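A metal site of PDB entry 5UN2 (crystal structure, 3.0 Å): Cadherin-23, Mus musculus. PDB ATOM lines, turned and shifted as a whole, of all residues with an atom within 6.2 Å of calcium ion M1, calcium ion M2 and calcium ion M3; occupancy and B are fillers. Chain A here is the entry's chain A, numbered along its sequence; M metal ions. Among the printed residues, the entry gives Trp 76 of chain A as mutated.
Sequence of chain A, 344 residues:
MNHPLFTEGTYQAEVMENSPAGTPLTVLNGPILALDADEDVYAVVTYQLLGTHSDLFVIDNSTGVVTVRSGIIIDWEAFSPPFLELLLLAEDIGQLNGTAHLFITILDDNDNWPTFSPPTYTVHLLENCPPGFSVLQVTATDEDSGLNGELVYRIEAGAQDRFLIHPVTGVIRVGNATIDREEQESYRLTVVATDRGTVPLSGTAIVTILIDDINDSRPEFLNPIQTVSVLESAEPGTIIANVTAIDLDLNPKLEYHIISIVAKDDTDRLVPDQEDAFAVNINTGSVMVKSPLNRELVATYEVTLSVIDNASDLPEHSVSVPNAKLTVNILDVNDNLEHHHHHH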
ATOM      1  N   GLU A  17     -13.493 -10.881  -1.170  1.00  0.00           N
ATOM      2  CA  GLU A  17     -13.845 -10.542   0.211  1.00  0.00           C
ATOM      3  C   GLU A  17     -13.114  -9.246   0.638  1.00  0.00           C
ATOM      4  O   GLU A  17     -12.044  -8.950   0.093  1.00  0.00           O
ATOM      5  CB  GLU A  17     -13.547 -11.721   1.178  1.00  0.00           C
ATOM      6  CG  GLU A  17     -12.057 -12.092   1.357  1.00  0.00           C
ATOM      7  CD  GLU A  17     -11.751 -12.935   2.608  1.00  0.00           C
ATOM      8  OE1 GLU A  17     -10.848 -13.805   2.530  1.00  0.00           O
ATOM      9  OE2 GLU A  17     -12.389 -12.729   3.676  1.00  0.00           O
ATOM     10  N   ASN A  18     -13.700  -8.500   1.585  1.00  0.00           N
ATOM     11  CA  ASN A  18     -13.154  -7.186   2.060  1.00  0.00           C
ATOM     12  C   ASN A  18     -13.123  -6.044   1.006  1.00  0.00           C
ATOM     13  O   ASN A  18     -12.400  -5.064   1.190  1.00  0.00           O
ATOM     14  CB  ASN A  18     -11.751  -7.333   2.691  1.00  0.00           C
ATOM     15  CG  ASN A  18     -11.608  -8.602   3.525  1.00  0.00           C
ATOM     16  OD1 ASN A  18     -12.458  -8.905   4.367  1.00  0.00           O
ATOM     17  ND2 ASN A  18     -10.527  -9.349   3.280  1.00  0.00           N
ATOM     18  N   ILE A  74     -17.793  -8.292   3.488  1.00  0.00           N
ATOM     19  CA  ILE A  74     -17.800  -9.614   2.832  1.00  0.00           C
ATOM     20  C   ILE A  74     -16.680 -10.460   3.471  1.00  0.00           C
ATOM     21  O   ILE A  74     -15.501 -10.105   3.359  1.00  0.00           O
ATOM     22  CB  ILE A  74     -17.507  -9.516   1.304  1.00  0.00           C
ATOM     23  CG1 ILE A  74     -18.406  -8.504   0.576  1.00  0.00           C
ATOM     24  CG2 ILE A  74     -17.606 -10.876   0.645  1.00  0.00           C
ATOM     25  CD1 ILE A  74     -19.890  -8.799   0.627  1.00  0.00           C
ATOM     26  N   ASP A  75     -17.040 -11.566   4.134  1.00  0.00           N
ATOM     27  CA  ASP A  75     -16.083 -12.445   4.845  1.00  0.00           C
ATOM     28  C   ASP A  75     -16.090 -13.869   4.246  1.00  0.00           C
ATOM     29  O   ASP A  75     -17.050 -14.623   4.447  1.00  0.00           O
ATOM     30  CB  ASP A  75     -16.469 -12.469   6.334  1.00  0.00           C
ATOM     31  CG  ASP A  75     -15.379 -13.035   7.222  1.00  0.00           C
ATOM     32  OD1 ASP A  75     -14.587 -13.886   6.779  1.00  0.00           O
ATOM     33  OD2 ASP A  75     -15.330 -12.623   8.387  1.00  0.00           O
ATOM     34  N   TRP A  76     -15.014 -14.238   3.531  1.00  0.00           N
ATOM     35  CA  TRP A  76     -14.879 -15.598   2.945  1.00  0.00           C
ATOM     36  C   TRP A  76     -14.971 -16.680   4.005  1.00  0.00           C
ATOM     37  O   TRP A  76     -15.598 -17.725   3.773  1.00  0.00           O
ATOM     38  CB  TRP A  76     -13.544 -15.754   2.209  1.00  0.00           C
ATOM     39  CG  TRP A  76     -13.454 -17.012   1.377  1.00  0.00           C
ATOM     40  CD1 TRP A  76     -13.752 -17.129   0.077  1.00  0.00           C
ATOM     41  CD2 TRP A  76     -13.026 -18.307   1.809  1.00  0.00           C
ATOM     42  NE1 TRP A  76     -13.541 -18.410  -0.353  1.00  0.00           N
ATOM     43  CE2 TRP A  76     -13.098 -19.163   0.696  1.00  0.00           C
ATOM     44  CE3 TRP A  76     -12.586 -18.840   3.027  1.00  0.00           C
ATOM     45  CZ2 TRP A  76     -12.768 -20.508   0.751  1.00  0.00           C
ATOM     46  CZ3 TRP A  76     -12.252 -20.181   3.090  1.00  0.00           C
ATOM     47  CH2 TRP A  76     -12.354 -21.001   1.955  1.00  0.00           C
ATOM     48  N   GLU A  77     -14.357 -16.422   5.156  1.00  0.00           N
ATOM     49  CA  GLU A  77     -14.302 -17.385   6.266  1.00  0.00           C
ATOM     50  C   GLU A  77     -15.652 -17.593   6.968  1.00  0.00           C
ATOM     51  O   GLU A  77     -15.787 -18.560   7.733  1.00  0.00           O
ATOM     52  CB  GLU A  77     -13.237 -16.978   7.296  1.00  0.00           C
ATOM     53  CG  GLU A  77     -11.792 -17.213   6.874  1.00  0.00           C
ATOM     54  CD  GLU A  77     -11.271 -16.160   5.908  1.00  0.00           C
ATOM     55  OE1 GLU A  77     -11.402 -14.940   6.190  1.00  0.00           O
ATOM     56  OE2 GLU A  77     -10.699 -16.554   4.871  1.00  0.00           O
ATOM     57  N   ALA A  78     -16.631 -16.707   6.717  1.00  0.00           N
ATOM     58  CA  ALA A  78     -17.973 -16.790   7.302  1.00  0.00           C
ATOM     59  C   ALA A  78     -19.049 -17.538   6.459  1.00  0.00           C
ATOM     60  O   ALA A  78     -20.144 -17.798   6.952  1.00  0.00           O
ATOM     61  CB  ALA A  78     -18.461 -15.388   7.652  1.00  0.00           C
ATOM     62  N   ASP A 108     -11.377 -15.746  -2.015  1.00  0.00           N
ATOM     63  CA  ASP A 108     -10.575 -15.720  -0.793  1.00  0.00           C
ATOM     64  C   ASP A 108      -9.440 -14.712  -0.931  1.00  0.00           C
ATOM     65  O   ASP A 108      -8.858 -14.596  -1.991  1.00  0.00           O
ATOM     66  CB  ASP A 108      -9.994 -17.119  -0.518  1.00  0.00           C
ATOM     67  CG  ASP A 108      -9.153 -17.173   0.751  1.00  0.00           C
ATOM     68  OD1 ASP A 108      -9.484 -16.466   1.720  1.00  0.00           O
ATOM     69  OD2 ASP A 108      -8.150 -17.942   0.776  1.00  0.00           O
ATOM     70  N   ASP A 109      -9.160 -13.975   0.151  1.00  0.00           N
ATOM     71  CA  ASP A 109      -7.956 -13.122   0.228  1.00  0.00           C
ATOM     72  C   ASP A 109      -7.136 -13.508   1.458  1.00  0.00           C
ATOM     73  O   ASP A 109      -7.697 -13.915   2.480  1.00  0.00           O
ATOM     74  CB  ASP A 109      -8.324 -11.630   0.292  1.00  0.00           C
ATOM     75  CG  ASP A 109      -7.091 -10.717   0.219  1.00  0.00           C
ATOM     76  OD1 ASP A 109      -6.140 -11.012  -0.532  1.00  0.00           O
ATOM     77  OD2 ASP A 109      -7.074  -9.696   0.930  1.00  0.00           O
ATOM     78  N   ASN A 110      -5.811 -13.387   1.348  1.00  0.00           N
ATOM     79  CA  ASN A 110      -4.902 -13.751   2.421  1.00  0.00           C
ATOM     80  C   ASN A 110      -5.038 -12.736   3.551  1.00  0.00           C
ATOM     81  O   ASN A 110      -4.293 -11.757   3.617  1.00  0.00           O
ATOM     82  CB  ASN A 110      -3.464 -13.818   1.887  1.00  0.00           C
ATOM     83  CG  ASN A 110      -2.488 -14.446   2.866  1.00  0.00           C
ATOM     84  OD1 ASN A 110      -2.877 -15.140   3.807  1.00  0.00           O
ATOM     85  ND2 ASN A 110      -1.209 -14.207   2.646  1.00  0.00           N
ATOM     86  N   ASP A 111      -6.020 -12.961   4.424  1.00  0.00           N
ATOM     87  CA  ASP A 111      -6.350 -12.017   5.496  1.00  0.00           C
ATOM     88  C   ASP A 111      -6.468 -12.663   6.881  1.00  0.00           C
ATOM     89  O   ASP A 111      -7.153 -12.129   7.762  1.00  0.00           O
ATOM     90  CB  ASP A 111      -7.638 -11.245   5.145  1.00  0.00           C
ATOM     91  CG  ASP A 111      -8.894 -12.136   5.109  1.00  0.00           C
ATOM     92  OD1 ASP A 111      -8.810 -13.374   5.130  1.00  0.00           O
ATOM     93  OD2 ASP A 111      -9.993 -11.564   5.045  1.00  0.00           O
ATOM     94  N   ASN A 112      -5.800 -13.806   7.079  1.00  0.00           N
ATOM     95  CA  ASN A 112      -5.663 -14.412   8.405  1.00  0.00           C
ATOM     96  C   ASN A 112      -4.194 -14.721   8.658  1.00  0.00           C
ATOM     97  O   ASN A 112      -3.504 -15.250   7.785  1.00  0.00           O
ATOM     98  CB  ASN A 112      -6.515 -15.676   8.553  1.00  0.00           C
ATOM     99  CG  ASN A 112      -7.993 -15.379   8.684  1.00  0.00           C
ATOM    100  OD1 ASN A 112      -8.567 -15.566   9.762  1.00  0.00           O
ATOM    101  ND2 ASN A 112      -8.619 -14.924   7.608  1.00  0.00           N
ATOM    102  N   TRP A 113      -3.745 -14.388   9.861  1.00  0.00           N
ATOM    103  CA  TRP A 113      -2.346 -14.487  10.247  1.00  0.00           C
ATOM    104  C   TRP A 113      -2.130 -15.887  10.813  1.00  0.00           C
ATOM    105  O   TRP A 113      -2.950 -16.336  11.620  1.00  0.00           O
ATOM    106  CB  TRP A 113      -2.006 -13.422  11.298  1.00  0.00           C
ATOM    107  CG  TRP A 113      -2.138 -12.015  10.774  1.00  0.00           C
ATOM    108  CD1 TRP A 113      -3.298 -11.339  10.460  1.00  0.00           C
ATOM    109  CD2 TRP A 113      -1.068 -11.100  10.495  1.00  0.00           C
ATOM    110  NE1 TRP A 113      -3.007 -10.071  10.001  1.00  0.00           N
ATOM    111  CE2 TRP A 113      -1.647  -9.903  10.013  1.00  0.00           C
ATOM    112  CE3 TRP A 113       0.335 -11.186  10.605  1.00  0.00           C
ATOM    113  CZ2 TRP A 113      -0.868  -8.783   9.645  1.00  0.00           C
ATOM    114  CZ3 TRP A 113       1.113 -10.080  10.234  1.00  0.00           C
ATOM    115  CH2 TRP A 113       0.508  -8.886   9.767  1.00  0.00           C
ATOM    116  N   PRO A 114      -1.056 -16.602  10.391  1.00  0.00           N
ATOM    117  CA  PRO A 114      -0.766 -17.906  10.998  1.00  0.00           C
ATOM    118  C   PRO A 114      -0.641 -17.789  12.497  1.00  0.00           C
ATOM    119  O   PRO A 114       0.249 -17.112  12.971  1.00  0.00           O
ATOM    120  CB  PRO A 114       0.588 -18.287  10.366  1.00  0.00           C
ATOM    121  CG  PRO A 114       0.616 -17.574   9.076  1.00  0.00           C
ATOM    122  CD  PRO A 114      -0.102 -16.281   9.321  1.00  0.00           C
ATOM    123  N   ASP A 142      -4.432 -21.578  10.472  1.00  0.00           N
ATOM    124  CA  ASP A 142      -4.709 -20.523   9.498  1.00  0.00           C
ATOM    125  C   ASP A 142      -6.109 -20.758   8.876  1.00  0.00           C
ATOM    126  O   ASP A 142      -6.349 -21.798   8.220  1.00  0.00           O
ATOM    127  CB  ASP A 142      -3.612 -20.509   8.428  1.00  0.00           C
ATOM    128  CG  ASP A 142      -3.524 -19.204   7.670  1.00  0.00           C
ATOM    129  OD1 ASP A 142      -4.557 -18.533   7.462  1.00  0.00           O
ATOM    130  OD2 ASP A 142      -2.405 -18.841   7.252  1.00  0.00           O
ATOM    131  N   GLU A 143      -6.995 -19.789   9.076  1.00  0.00           N
ATOM    132  CA  GLU A 143      -8.371 -19.888   8.574  1.00  0.00           C
ATOM    133  C   GLU A 143      -8.523 -19.521   7.102  1.00  0.00           C
ATOM    134  O   GLU A 143      -9.627 -19.595   6.568  1.00  0.00           O
ATOM    135  CB  GLU A 143      -9.336 -19.047   9.423  1.00  0.00           C
ATOM    136  CG  GLU A 143      -9.271 -19.330  10.924  1.00  0.00           C
ATOM    137  CD  GLU A 143      -9.332 -20.810  11.257  1.00  0.00           C
ATOM    138  OE1 GLU A 143     -10.386 -21.444  11.041  1.00  0.00           O
ATOM    139  OE2 GLU A 143      -8.301 -21.346  11.731  1.00  0.00           O
ATOM    140  N   ASP A 144      -7.427 -19.138   6.443  1.00  0.00           N
ATOM    141  CA  ASP A 144      -7.426 -18.945   4.994  1.00  0.00           C
ATOM    142  C   ASP A 144      -7.464 -20.285   4.248  1.00  0.00           C
ATOM    143  O   ASP A 144      -7.361 -21.342   4.866  1.00  0.00           O
ATOM    144  CB  ASP A 144      -6.188 -18.138   4.566  1.00  0.00           C
ATOM    145  CG  ASP A 144      -6.266 -16.693   4.957  1.00  0.00           C
ATOM    146  OD1 ASP A 144      -7.350 -16.094   4.787  1.00  0.00           O
ATOM    147  OD2 ASP A 144      -5.241 -16.130   5.397  1.00  0.00           O
ATOM    148  N   SER A 145      -7.613 -20.190   2.921  1.00  0.00           N
ATOM    149  CA  SER A 145      -7.712 -21.352   2.033  1.00  0.00           C
ATOM    150  C   SER A 145      -6.560 -21.450   1.051  1.00  0.00           C
ATOM    151  O   SER A 145      -5.944 -20.432   0.708  1.00  0.00           O
ATOM    152  CB  SER A 145      -9.009 -21.289   1.231  1.00  0.00           C
ATOM    153  OG  SER A 145      -8.889 -20.393   0.124  1.00  0.00           O
ATOM    154  N   LEU A 147      -3.195 -21.835  -0.801  1.00  0.00           N
ATOM    155  CA  LEU A 147      -1.844 -21.422  -0.435  1.00  0.00           C
ATOM    156  C   LEU A 147      -1.829 -20.406   0.692  1.00  0.00           C
ATOM    157  O   LEU A 147      -0.848 -20.335   1.428  1.00  0.00           O
ATOM    158  CB  LEU A 147      -1.081 -20.888  -1.641  1.00  0.00           C
ATOM    159  CG  LEU A 147      -0.628 -21.937  -2.667  1.00  0.00           C
ATOM    160  CD1 LEU A 147       0.049 -21.229  -3.826  1.00  0.00           C
ATOM    161  CD2 LEU A 147       0.294 -22.990  -2.044  1.00  0.00           C
ATOM    162  N   ASN A 148      -2.905 -19.651   0.850  1.00  0.00           N
ATOM    163  CA  ASN A 148      -2.986 -18.644   1.916  1.00  0.00           C
ATOM    164  C   ASN A 148      -3.103 -19.254   3.329  1.00  0.00           C
ATOM    165  O   ASN A 148      -2.920 -18.548   4.326  1.00  0.00           O
ATOM    166  CB  ASN A 148      -4.157 -17.689   1.654  1.00  0.00           C
ATOM    167  CG  ASN A 148      -4.170 -17.141   0.248  1.00  0.00           C
ATOM    168  OD1 ASN A 148      -3.126 -16.835  -0.355  1.00  0.00           O
ATOM    169  ND2 ASN A 148      -5.372 -17.006  -0.309  1.00  0.00           N
ATOM    170  N   GLY A 149      -3.453 -20.537   3.404  1.00  0.00           N
ATOM    171  CA  GLY A 149      -3.446 -21.319   4.642  1.00  0.00           C
ATOM    172  C   GLY A 149      -2.279 -22.267   4.821  1.00  0.00           C
ATOM    173  O   GLY A 149      -1.949 -22.627   5.953  1.00  0.00           O
ATOM    174  N   LEU A 151       1.165 -23.449   5.521  1.00  0.00           N
ATOM    175  CA  LEU A 151       2.174 -22.839   6.403  1.00  0.00           C
ATOM    176  C   LEU A 151       3.565 -23.449   6.281  1.00  0.00           C
ATOM    177  O   LEU A 151       3.710 -24.643   6.066  1.00  0.00           O
ATOM    178  CB  LEU A 151       1.736 -22.943   7.868  1.00  0.00           C
ATOM    179  CG  LEU A 151       0.463 -22.247   8.346  1.00  0.00           C
ATOM    180  CD1 LEU A 151       0.361 -22.371   9.854  1.00  0.00           C
ATOM    181  CD2 LEU A 151       0.432 -20.780   7.939  1.00  0.00           C
ATOM    182  N   ASP A 195       2.686 -17.981   5.935  1.00  0.00           N
ATOM    183  CA  ASP A 195       1.815 -18.514   4.872  1.00  0.00           C
ATOM    184  C   ASP A 195       2.438 -18.290   3.478  1.00  0.00           C
ATOM    185  O   ASP A 195       3.381 -17.493   3.335  1.00  0.00           O
ATOM    186  CB  ASP A 195       0.385 -17.976   4.973  1.00  0.00           C
ATOM    187  CG  ASP A 195       0.277 -16.490   4.674  1.00  0.00           C
ATOM    188  OD1 ASP A 195       0.540 -16.068   3.537  1.00  0.00           O
ATOM    189  OD2 ASP A 195      -0.138 -15.731   5.574  1.00  0.00           O
ATOM    190  N   LEU A 201       1.644 -13.422   5.119  1.00  0.00           N
ATOM    191  CA  LEU A 201       1.659 -13.081   6.539  1.00  0.00           C
ATOM    192  C   LEU A 201       2.382 -14.159   7.353  1.00  0.00           C
ATOM    193  O   LEU A 201       2.558 -15.291   6.893  1.00  0.00           O
ATOM    194  CB  LEU A 201       0.222 -12.862   7.047  1.00  0.00           C
ATOM    195  CG  LEU A 201      -0.634 -11.895   6.209  1.00  0.00           C
ATOM    196  CD1 LEU A 201      -2.083 -11.935   6.649  1.00  0.00           C
ATOM    197  CD2 LEU A 201      -0.082 -10.476   6.275  1.00  0.00           C
HETATM  198 CA    CA M   1      -2.835 -16.512   5.791  1.00  0.00          CA
HETATM  199 CA    CA M   2      -9.293 -15.208   3.689  1.00  0.00          CA
HETATM  200 CA    CA M   3     -12.088 -12.596   6.013  1.00  0.00          CA
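Calcium ion M2 is bound by OE2 of Glu 77, OD1 of Asp 108, OD1 of Asp 111, O of Asp 109, OE1 of Glu 17 and OD1 of Asp 144.
OD2 of Asp 108 sits at hydrogen-bond distance from ND2 of Asn 148, at 3.1 Å.
The side-chain carboxylate (OE1) of Glu 77 lies close to the side-chain amide nitrogen (ND2) of Asn 112, at 3.1 Å.
The backbone NH (N) of Glu 77 sits at hydrogen-bond distance from the side-chain carboxylate (OD1) of Asp 75 (3.0 Å).
OE2 of Glu 17 sits close to N of Trp 76, 3.0 Å away.
The side-chain amide nitrogen (ND2) of Asn 112 lies close to the side-chain carboxylate (OD1) of Asp 111 (2.9 Å).
OD2 of Asp 108 sits at hydrogen-bond distance from OG of Ser 145, at 2.6 Å.
The backbone NH (N) of Ala 78 is in hydrogen-bond range of the side-chain carboxylate (OD1) of Asp 75 (3.5 Å).
N of Asp 195 is in hydrogen-bond range of O of Leu 201.
Calcium ion M1 is bound by the side-chain amide oxygen of Asn 110 (2.4 Å), the backbone carbonyl oxygen of Asn 112 (2.5 Å), the side-chain carboxylate of Asp 144 (2.5 Å), the backbone carbonyl oxygen of Asn 148 (2.5 Å), the side-chain carboxylate of Asp 142 (2.8 Å) and the side-chain carboxylate of Asp 195 (2.8 Å).
Calcium ion M1 has six donor atoms within binding distance.
Slightly farther from calcium ion M1 lies OD1 of Asp 142 (3.1 Å).
Calcium ion M3 is bound by the side-chain carboxylate of Glu 17 (2.4 Å), the side-chain carboxylate of Glu 77 (2.4 Å) and the side-chain carboxylate of Asp 111 (2.5 Å).
Calcium ion M3 has three donor atoms within binding distance.
Slightly farther from calcium ion M3 lies OD1 of Asp 75 (2.9 Å).
Four residues have an atom within 4 Å of calcium ion M3: Glu 17, Asp 75, Glu 77 and Asp 111.
Within 4 Å of calcium ion M1: Asn 110, Asn 112, Asp 142, Asp 144, Asn 148 and Asp 195.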
